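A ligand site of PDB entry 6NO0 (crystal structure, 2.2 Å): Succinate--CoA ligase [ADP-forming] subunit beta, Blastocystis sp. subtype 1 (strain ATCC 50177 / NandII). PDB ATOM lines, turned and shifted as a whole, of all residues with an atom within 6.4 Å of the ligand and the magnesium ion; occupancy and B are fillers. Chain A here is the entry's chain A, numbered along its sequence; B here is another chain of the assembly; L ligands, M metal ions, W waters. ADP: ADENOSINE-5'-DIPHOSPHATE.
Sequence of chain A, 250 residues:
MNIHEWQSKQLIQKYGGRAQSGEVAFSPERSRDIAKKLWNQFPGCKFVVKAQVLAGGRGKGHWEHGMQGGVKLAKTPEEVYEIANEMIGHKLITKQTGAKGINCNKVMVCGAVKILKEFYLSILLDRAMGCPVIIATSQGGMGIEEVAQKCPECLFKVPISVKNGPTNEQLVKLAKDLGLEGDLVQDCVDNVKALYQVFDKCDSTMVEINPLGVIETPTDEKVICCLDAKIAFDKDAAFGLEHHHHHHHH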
ATOM      1  N   GLU A   5      22.085  24.440  -3.275  1.00  0.00           N
ATOM      2  CA  GLU A   5      22.067  23.090  -2.725  1.00  0.00           C
ATOM      3  C   GLU A   5      22.606  23.053  -1.292  1.00  0.00           C
ATOM      4  O   GLU A   5      21.920  22.591  -0.371  1.00  0.00           O
ATOM      5  CB  GLU A   5      22.873  22.159  -3.636  1.00  0.00           C
ATOM      6  CG  GLU A   5      23.004  20.734  -3.131  1.00  0.00           C
ATOM      7  CD  GLU A   5      23.933  19.898  -3.987  1.00  0.00           C
ATOM      8  OE1 GLU A   5      24.609  20.471  -4.873  1.00  0.00           O
ATOM      9  OE2 GLU A   5      24.008  18.673  -3.775  1.00  0.00           O
ATOM     10  N   LYS A   9      20.767  21.818   2.219  1.00  0.00           N
ATOM     11  CA  LYS A   9      21.177  20.648   2.995  1.00  0.00           C
ATOM     12  C   LYS A   9      21.539  21.023   4.429  1.00  0.00           C
ATOM     13  O   LYS A   9      21.227  20.284   5.361  1.00  0.00           O
ATOM     14  CB  LYS A   9      22.349  19.948   2.310  1.00  0.00           C
ATOM     15  CG  LYS A   9      22.018  19.357   0.953  1.00  0.00           C
ATOM     16  CD  LYS A   9      23.146  18.485   0.438  1.00  0.00           C
ATOM     17  CE  LYS A   9      22.809  17.848  -0.898  1.00  0.00           C
ATOM     18  NZ  LYS A   9      23.990  17.140  -1.489  1.00  0.00           N
ATOM     19  N   GLN A  20      24.281  15.238   2.718  1.00  0.00           N
ATOM     20  CA  GLN A  20      25.692  15.442   2.440  1.00  0.00           C
ATOM     21  C   GLN A  20      25.872  16.883   1.993  1.00  0.00           C
ATOM     22  O   GLN A  20      25.886  17.207   0.804  1.00  0.00           O
ATOM     23  CB  GLN A  20      26.201  14.465   1.379  1.00  0.00           C
ATOM     24  CG  GLN A  20      27.707  14.538   1.165  1.00  0.00           C
ATOM     25  CD  GLN A  20      28.196  13.626   0.057  1.00  0.00           C
ATOM     26  OE1 GLN A  20      27.626  13.590  -1.030  1.00  0.00           O
ATOM     27  NE2 GLN A  20      29.245  12.878   0.338  1.00  0.00           N
ATOM     28  N   VAL A  48      33.775  14.426  -5.082  1.00  0.00           N
ATOM     29  CA  VAL A  48      32.807  14.900  -6.059  1.00  0.00           C
ATOM     30  C   VAL A  48      32.736  16.418  -5.943  1.00  0.00           C
ATOM     31  O   VAL A  48      32.564  16.955  -4.845  1.00  0.00           O
ATOM     32  CB  VAL A  48      31.420  14.275  -5.839  1.00  0.00           C
ATOM     33  CG1 VAL A  48      30.444  14.756  -6.910  1.00  0.00           C
ATOM     34  CG2 VAL A  48      31.508  12.759  -5.847  1.00  0.00           C
ATOM     35  N   LYS A  50      30.682  19.711  -7.096  1.00  0.00           N
ATOM     36  CA  LYS A  50      29.330  20.025  -7.539  1.00  0.00           C
ATOM     37  C   LYS A  50      29.213  21.539  -7.674  1.00  0.00           C
ATOM     38  O   LYS A  50      29.293  22.276  -6.679  1.00  0.00           O
ATOM     39  CB  LYS A  50      28.291  19.485  -6.557  1.00  0.00           C
ATOM     40  CG  LYS A  50      28.471  18.013  -6.219  1.00  0.00           C
ATOM     41  CD  LYS A  50      27.385  17.496  -5.294  1.00  0.00           C
ATOM     42  CE  LYS A  50      26.086  17.224  -6.043  1.00  0.00           C
ATOM     43  NZ  LYS A  50      25.046  16.664  -5.140  1.00  0.00           N
ATOM     44  N   ALA A  55      20.230  26.452 -10.877  1.00  0.00           N
ATOM     45  CA  ALA A  55      19.731  25.831 -12.095  1.00  0.00           C
ATOM     46  C   ALA A  55      19.876  24.318 -11.975  1.00  0.00           C
ATOM     47  O   ALA A  55      20.786  23.828 -11.302  1.00  0.00           O
ATOM     48  CB  ALA A  55      20.482  26.336 -13.334  1.00  0.00           C
ATOM     49  N   GLY A  56      18.974  23.601 -12.639  1.00  0.00           N
ATOM     50  CA  GLY A  56      18.977  22.149 -12.630  1.00  0.00           C
ATOM     51  C   GLY A  56      19.691  21.557 -13.829  1.00  0.00           C
ATOM     52  O   GLY A  56      20.101  22.256 -14.760  1.00  0.00           O
ATOM     53  N   GLY A  57      19.850  20.238 -13.798  1.00  0.00           N
ATOM     54  CA  GLY A  57      20.508  19.528 -14.872  1.00  0.00           C
ATOM     55  C   GLY A  57      22.011  19.739 -14.925  1.00  0.00           C
ATOM     56  O   GLY A  57      22.583  19.751 -16.021  1.00  0.00           O
ATOM     57  N   ARG A  58      22.654  19.906 -13.770  1.00  0.00           N
ATOM     58  CA  ARG A  58      24.096  20.129 -13.758  1.00  0.00           C
ATOM     59  C   ARG A  58      24.855  18.913 -14.260  1.00  0.00           C
ATOM     60  O   ARG A  58      25.844  19.054 -14.995  1.00  0.00           O
ATOM     61  CB  ARG A  58      24.557  20.480 -12.335  1.00  0.00           C
ATOM     62  CG  ARG A  58      23.922  21.738 -11.768  1.00  0.00           C
ATOM     63  CD  ARG A  58      24.303  21.906 -10.296  1.00  0.00           C
ATOM     64  NE  ARG A  58      23.780  20.831  -9.471  1.00  0.00           N
ATOM     65  CZ  ARG A  58      24.040  20.681  -8.179  1.00  0.00           C
ATOM     66  NH1 ARG A  58      24.832  21.550  -7.547  1.00  0.00           N
ATOM     67  NH2 ARG A  58      23.515  19.671  -7.504  1.00  0.00           N
ATOM     68  N   GLY A  59      24.407  17.707 -13.893  1.00  0.00           N
ATOM     69  CA  GLY A  59      25.158  16.511 -14.245  1.00  0.00           C
ATOM     70  C   GLY A  59      25.377  16.355 -15.737  1.00  0.00           C
ATOM     71  O   GLY A  59      26.431  15.887 -16.169  1.00  0.00           O
ATOM     72  N   LYS A  60      24.383  16.746 -16.537  1.00  0.00           N
ATOM     73  CA  LYS A  60      24.453  16.598 -17.991  1.00  0.00           C
ATOM     74  C   LYS A  60      24.711  17.912 -18.702  1.00  0.00           C
ATOM     75  O   LYS A  60      24.619  17.961 -19.936  1.00  0.00           O
ATOM     76  CB  LYS A  60      23.168  15.954 -18.520  1.00  0.00           C
ATOM     77  CG  LYS A  60      22.903  14.564 -17.954  1.00  0.00           C
ATOM     78  CD  LYS A  60      21.611  13.993 -18.502  1.00  0.00           C
ATOM     79  CE  LYS A  60      21.317  12.623 -17.907  1.00  0.00           C
ATOM     80  NZ  LYS A  60      20.065  12.031 -18.449  1.00  0.00           N
ATOM     81  N   VAL A  71      28.591  18.289 -12.134  1.00  0.00           N
ATOM     82  CA  VAL A  71      28.838  17.412 -11.003  1.00  0.00           C
ATOM     83  C   VAL A  71      29.838  16.369 -11.491  1.00  0.00           C
ATOM     84  O   VAL A  71      29.467  15.439 -12.220  1.00  0.00           O
ATOM     85  CB  VAL A  71      27.556  16.742 -10.477  1.00  0.00           C
ATOM     86  CG1 VAL A  71      27.885  15.738  -9.384  1.00  0.00           C
ATOM     87  CG2 VAL A  71      26.574  17.802  -9.984  1.00  0.00           C
ATOM     88  N   LEU A  73      33.313  13.757 -10.788  1.00  0.00           N
ATOM     89  CA  LEU A  73      34.083  12.969  -9.833  1.00  0.00           C
ATOM     90  C   LEU A  73      35.574  13.266  -9.992  1.00  0.00           C
ATOM     91  O   LEU A  73      36.063  13.503 -11.103  1.00  0.00           O
ATOM     92  CB  LEU A  73      33.815  11.473 -10.057  1.00  0.00           C
ATOM     93  CG  LEU A  73      34.576  10.460  -9.196  1.00  0.00           C
ATOM     94  CD1 LEU A  73      33.993  10.381  -7.796  1.00  0.00           C
ATOM     95  CD2 LEU A  73      34.550   9.100  -9.874  1.00  0.00           C
ATOM     96  N   CYS A 110      32.444  17.338  -1.952  1.00  0.00           N
ATOM     97  CA  CYS A 110      31.949  16.234  -1.148  1.00  0.00           C
ATOM     98  C   CYS A 110      32.818  15.002  -1.355  1.00  0.00           C
ATOM     99  O   CYS A 110      33.529  14.880  -2.355  1.00  0.00           O
ATOM    100  CB  CYS A 110      30.491  15.893  -1.483  1.00  0.00           C
ATOM    101  SG  CYS A 110      29.407  17.320  -1.638  1.00  0.00           S
ATOM    102  N   GLY A 111      32.759  14.098  -0.383  1.00  0.00           N
ATOM    103  CA  GLY A 111      33.380  12.793  -0.549  1.00  0.00           C
ATOM    104  C   GLY A 111      32.494  11.883  -1.382  1.00  0.00           C
ATOM    105  O   GLY A 111      31.272  11.911  -1.287  1.00  0.00           O
ATOM    106  N   ALA A 112      33.140  11.071  -2.219  1.00  0.00           N
ATOM    107  CA  ALA A 112      32.401  10.117  -3.036  1.00  0.00           C
ATOM    108  C   ALA A 112      31.890   8.988  -2.166  1.00  0.00           C
ATOM    109  O   ALA A 112      32.641   8.407  -1.369  1.00  0.00           O
ATOM    110  CB  ALA A 112      33.282   9.587  -4.156  1.00  0.00           C
ATOM    111  N   VAL A 113      30.606   8.655  -2.324  1.00  0.00           N
ATOM    112  CA  VAL A 113      29.979   7.593  -1.555  1.00  0.00           C
ATOM    113  C   VAL A 113      29.341   6.594  -2.517  1.00  0.00           C
ATOM    114  O   VAL A 113      29.003   6.931  -3.654  1.00  0.00           O
ATOM    115  CB  VAL A 113      28.925   8.129  -0.558  1.00  0.00           C
ATOM    116  CG1 VAL A 113      29.602   8.964   0.522  1.00  0.00           C
ATOM    117  CG2 VAL A 113      27.867   8.947  -1.295  1.00  0.00           C
ATOM    118  N   LYS A 114      29.179   5.369  -2.041  1.00  0.00           N
ATOM    119  CA  LYS A 114      28.509   4.326  -2.807  1.00  0.00           C
ATOM    120  C   LYS A 114      26.998   4.511  -2.662  1.00  0.00           C
ATOM    121  O   LYS A 114      26.461   4.485  -1.549  1.00  0.00           O
ATOM    122  CB  LYS A 114      28.936   2.946  -2.310  1.00  0.00           C
ATOM    123  CG  LYS A 114      28.583   1.805  -3.250  1.00  0.00           C
ATOM    124  CD  LYS A 114      29.135   0.486  -2.730  1.00  0.00           C
ATOM    125  CE  LYS A 114      28.683  -0.687  -3.581  1.00  0.00           C
ATOM    126  NZ  LYS A 114      29.177  -1.987  -3.055  1.00  0.00           N
ATOM    127  N   ILE A 115      26.324   4.704  -3.794  1.00  0.00           N
ATOM    128  CA  ILE A 115      24.871   4.922  -3.823  1.00  0.00           C
ATOM    129  C   ILE A 115      24.205   3.622  -4.243  1.00  0.00           C
ATOM    130  O   ILE A 115      24.506   3.076  -5.312  1.00  0.00           O
ATOM    131  CB  ILE A 115      24.505   6.078  -4.773  1.00  0.00           C
ATOM    132  CG1 ILE A 115      25.340   7.327  -4.452  1.00  0.00           C
ATOM    133  CG2 ILE A 115      23.018   6.386  -4.659  1.00  0.00           C
ATOM    134  CD1 ILE A 115      25.132   8.456  -5.431  1.00  0.00           C
ATOM    135  N   GLU A 118      18.243   5.453  -5.439  1.00  0.00           N
ATOM    136  CA  GLU A 118      17.932   6.879  -5.552  1.00  0.00           C
ATOM    137  C   GLU A 118      16.425   7.044  -5.661  1.00  0.00           C
ATOM    138  O   GLU A 118      15.800   6.510  -6.589  1.00  0.00           O
ATOM    139  CB  GLU A 118      18.629   7.504  -6.764  1.00  0.00           C
ATOM    140  CG  GLU A 118      20.150   7.537  -6.652  1.00  0.00           C
ATOM    141  CD  GLU A 118      20.791   8.414  -7.700  1.00  0.00           C
ATOM    142  OE1 GLU A 118      20.084   8.895  -8.599  1.00  0.00           O
ATOM    143  OE2 GLU A 118      22.023   8.623  -7.616  1.00  0.00           O
ATOM    144  N   ASN A 210      15.929  15.349  -4.837  1.00  0.00           N
ATOM    145  CA  ASN A 210      16.081  14.645  -6.103  1.00  0.00           C
ATOM    146  C   ASN A 210      17.571  14.469  -6.377  1.00  0.00           C
ATOM    147  O   ASN A 210      18.208  15.335  -6.989  1.00  0.00           O
ATOM    148  CB  ASN A 210      15.409  15.395  -7.246  1.00  0.00           C
ATOM    149  CG  ASN A 210      15.429  14.620  -8.550  1.00  0.00           C
ATOM    150  OD1 ASN A 210      15.415  13.393  -8.553  1.00  0.00           O
ATOM    151  ND2 ASN A 210      15.481  15.334  -9.668  1.00  0.00           N
ATOM    152  N   PRO A 211      18.160  13.332  -5.961  1.00  0.00           N
ATOM    153  CA  PRO A 211      17.566  12.150  -5.343  1.00  0.00           C
ATOM    154  C   PRO A 211      17.681  12.093  -3.822  1.00  0.00           C
ATOM    155  O   PRO A 211      18.631  12.624  -3.245  1.00  0.00           O
ATOM    156  CB  PRO A 211      18.384  11.010  -5.957  1.00  0.00           C
ATOM    157  CG  PRO A 211      19.757  11.595  -6.062  1.00  0.00           C
ATOM    158  CD  PRO A 211      19.574  13.080  -6.327  1.00  0.00           C
ATOM    159  N   LEU A 227      21.017  13.479  -1.230  1.00  0.00           N
ATOM    160  CA  LEU A 227      22.145  13.744  -2.112  1.00  0.00           C
ATOM    161  C   LEU A 227      21.960  15.016  -2.923  1.00  0.00           C
ATOM    162  O   LEU A 227      22.926  15.507  -3.511  1.00  0.00           O
ATOM    163  CB  LEU A 227      22.360  12.556  -3.054  1.00  0.00           C
ATOM    164  CG  LEU A 227      22.626  11.220  -2.364  1.00  0.00           C
ATOM    165  CD1 LEU A 227      22.648  10.090  -3.373  1.00  0.00           C
ATOM    166  CD2 LEU A 227      23.918  11.264  -1.574  1.00  0.00           C
ATOM    167  N   ASP A 228      20.747  15.555  -2.970  1.00  0.00           N
ATOM    168  CA  ASP A 228      20.468  16.841  -3.592  1.00  0.00           C
ATOM    169  C   ASP A 228      19.293  17.459  -2.850  1.00  0.00           C
ATOM    170  O   ASP A 228      18.549  16.768  -2.152  1.00  0.00           O
ATOM    171  CB  ASP A 228      20.159  16.689  -5.089  1.00  0.00           C
ATOM    172  CG  ASP A 228      20.187  18.010  -5.837  1.00  0.00           C
ATOM    173  OD1 ASP A 228      20.524  19.034  -5.220  1.00  0.00           O
ATOM    174  OD2 ASP A 228      19.860  18.014  -7.045  1.00  0.00           O
ATOM    175  N   ALA A 229      19.127  18.769  -3.017  1.00  0.00           N
ATOM    176  CA  ALA A 229      18.074  19.454  -2.295  1.00  0.00           C
ATOM    177  C   ALA A 229      17.745  20.766  -2.987  1.00  0.00           C
ATOM    178  O   ALA A 229      18.634  21.483  -3.449  1.00  0.00           O
ATOM    179  CB  ALA A 229      18.479  19.713  -0.831  1.00  0.00           C
ATOM    180  N   GLN B  41      30.469  15.210   5.229  1.00  0.00           N
ATOM    181  CA  GLN B  41      31.174  14.595   4.118  1.00  0.00           C
ATOM    182  C   GLN B  41      30.841  13.121   3.940  1.00  0.00           C
ATOM    183  O   GLN B  41      30.719  12.650   2.799  1.00  0.00           O
ATOM    184  CB  GLN B  41      32.683  14.749   4.314  1.00  0.00           C
ATOM    185  CG  GLN B  41      33.176  16.180   4.233  1.00  0.00           C
ATOM    186  CD  GLN B  41      33.093  16.736   2.831  1.00  0.00           C
ATOM    187  OE1 GLN B  41      32.566  16.092   1.926  1.00  0.00           O
ATOM    188  NE2 GLN B  41      33.631  17.935   2.632  1.00  0.00           N
HETATM  189  PB  ADP L   1      21.596  17.747 -10.468  1.00  0.00           P
HETATM  190  O1B ADP L   1      21.182  19.172 -10.311  1.00  0.00           O
HETATM  191  O2B ADP L   1      22.238  17.464 -11.839  1.00  0.00           O
HETATM  192  O3B ADP L   1      20.436  16.764 -10.274  1.00  0.00           O
HETATM  193  PA  ADP L   1      22.788  16.201  -8.293  1.00  0.00           P
HETATM  194  O1A ADP L   1      23.025  16.749  -6.948  1.00  0.00           O
HETATM  195  O2A ADP L   1      21.510  15.360  -8.424  1.00  0.00           O
HETATM  196  O3A ADP L   1      22.698  17.351  -9.391  1.00  0.00           O
HETATM  197  O5' ADP L   1      24.002  15.271  -8.763  1.00  0.00           O
HETATM  198  C5' ADP L   1      24.029  14.439  -9.939  1.00  0.00           C
HETATM  199  C4' ADP L   1      24.169  13.001  -9.522  1.00  0.00           C
HETATM  200  O4' ADP L   1      25.450  12.792  -8.899  1.00  0.00           O
HETATM  201  C3' ADP L   1      23.168  12.515  -8.478  1.00  0.00           C
HETATM  202  O3' ADP L   1      21.938  12.156  -9.086  1.00  0.00           O
HETATM  203  C2' ADP L   1      23.887  11.303  -7.883  1.00  0.00           C
HETATM  204  O2' ADP L   1      23.622  10.114  -8.627  1.00  0.00           O
HETATM  205  C1' ADP L   1      25.371  11.687  -8.005  1.00  0.00           C
HETATM  206  N9  ADP L   1      25.993  12.074  -6.748  1.00  0.00           N
HETATM  207  C8  ADP L   1      25.671  13.135  -5.940  1.00  0.00           C
HETATM  208  N7  ADP L   1      26.399  13.224  -4.857  1.00  0.00           N
HETATM  209  C5  ADP L   1      27.277  12.154  -4.953  1.00  0.00           C
HETATM  210  C6  ADP L   1      28.309  11.692  -4.113  1.00  0.00           C
HETATM  211  N6  ADP L   1      28.654  12.283  -2.964  1.00  0.00           N
HETATM  212  N1  ADP L   1      28.986  10.593  -4.505  1.00  0.00           N
HETATM  213  C2  ADP L   1      28.641  10.003  -5.654  1.00  0.00           C
HETATM  214  N3  ADP L   1      27.695  10.342  -6.525  1.00  0.00           N
HETATM  215  C4  ADP L   1      27.034  11.433  -6.109  1.00  0.00           C
HETATM  216 MG    MG M   1      19.486  16.384  -8.331  1.00  0.00          MG
HETATM  217  O   HOH W   1      25.856  15.391  -2.529  1.00  0.00           O
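The magnesium ion is bound by OD2 of Asp 228 (2.1 Å), O of Asn 210 (2.1 Å), O3B of the ligand (2.2 Å) and O2A of the ligand (2.3 Å).
OE2 of Glu 118 is in hydrogen-bond range of O2' of the ligand (2.4 Å).
OE1 of Gln 20 sits at hydrogen-bond distance from N6 of the ligand, 2.6 Å away.
NZ of Lys 50 is in salt-bridge range of O1A of the ligand, at 2.7 Å.
The backbone NH of Gly 59 sits at hydrogen-bond distance from an oxygen (O2B) of the ligand.
The backbone NH of Arg 58 lies within hydrogen-bond range of an oxygen (O2B) of the ligand.
NH2 of Arg 58 lies within salt-bridge range of O1A of the ligand (3.0 Å).
The backbone carbonyl oxygen (O) of Gly 111 sits at hydrogen-bond distance from a nitrogen (N6) of the ligand, at 3.1 Å.
A nitrogen (N1) of the ligand sits at hydrogen-bond distance from the backbone NH of Val 113 (3.3 Å).
NZ of Lys 9 lies within hydrogen-bond range of O of Gln 20 (3.0 Å).
NE2 of Gln 20 lies within hydrogen-bond range of O of Gln 41 of chain B (2.9 Å).
The side-chain amino group (NZ) of Lys 50 is in hydrogen-bond range of the backbone carbonyl oxygen (O) of Leu 227.
The side-chain carboxylate (OE2) of Glu 5 lies within salt-bridge range of the side-chain amino group (NZ) of Lys 50, 2.6 Å away.
The side-chain amide oxygen (OE1) of Gln 41 of chain B lies within hydrogen-bond range of the backbone NH (N) of Gly 111, at 3.1 Å.
The backbone NH of Val 48 is in hydrogen-bond range of the backbone carbonyl oxygen of Cys 110, at 2.8 Å.
The backbone carbonyl oxygen of Leu 227 sits at hydrogen-bond distance from the side-chain amino group of Lys 9 (2.8 Å).
OE2 of Glu 5 lies within salt-bridge range of NZ of Lys 9, at 2.8 Å.
Pro 211 touches the magnesium ion.
Within 4 Å of the magnesium ion: Asn 210, Pro 211 and Asp 228.
The nearest printed residue that does not touch the magnesium ion is Arg 58 (5.3 Å).
Residues that only touch the ligand: Glu 5 (3.8 Å), Val 48 (3.6 Å), Gly 57 (3.8 Å), Val 71 (3.8 Å), Ala 112 (3.7 Å), Ile 115 (3.4 Å), Pro 211 (3.7 Å) and Leu 227 (3.7 Å).
Hydrophobic or aromatic side chains that line the ligand: Val 48, Val 71, Val 113, Ile 115 and Pro 211.
Of the 26 residues printed, 17 come within 4 Å of the ligand.
The nearest printed residue that does not touch the ligand is Cys 110 (4.3 Å).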
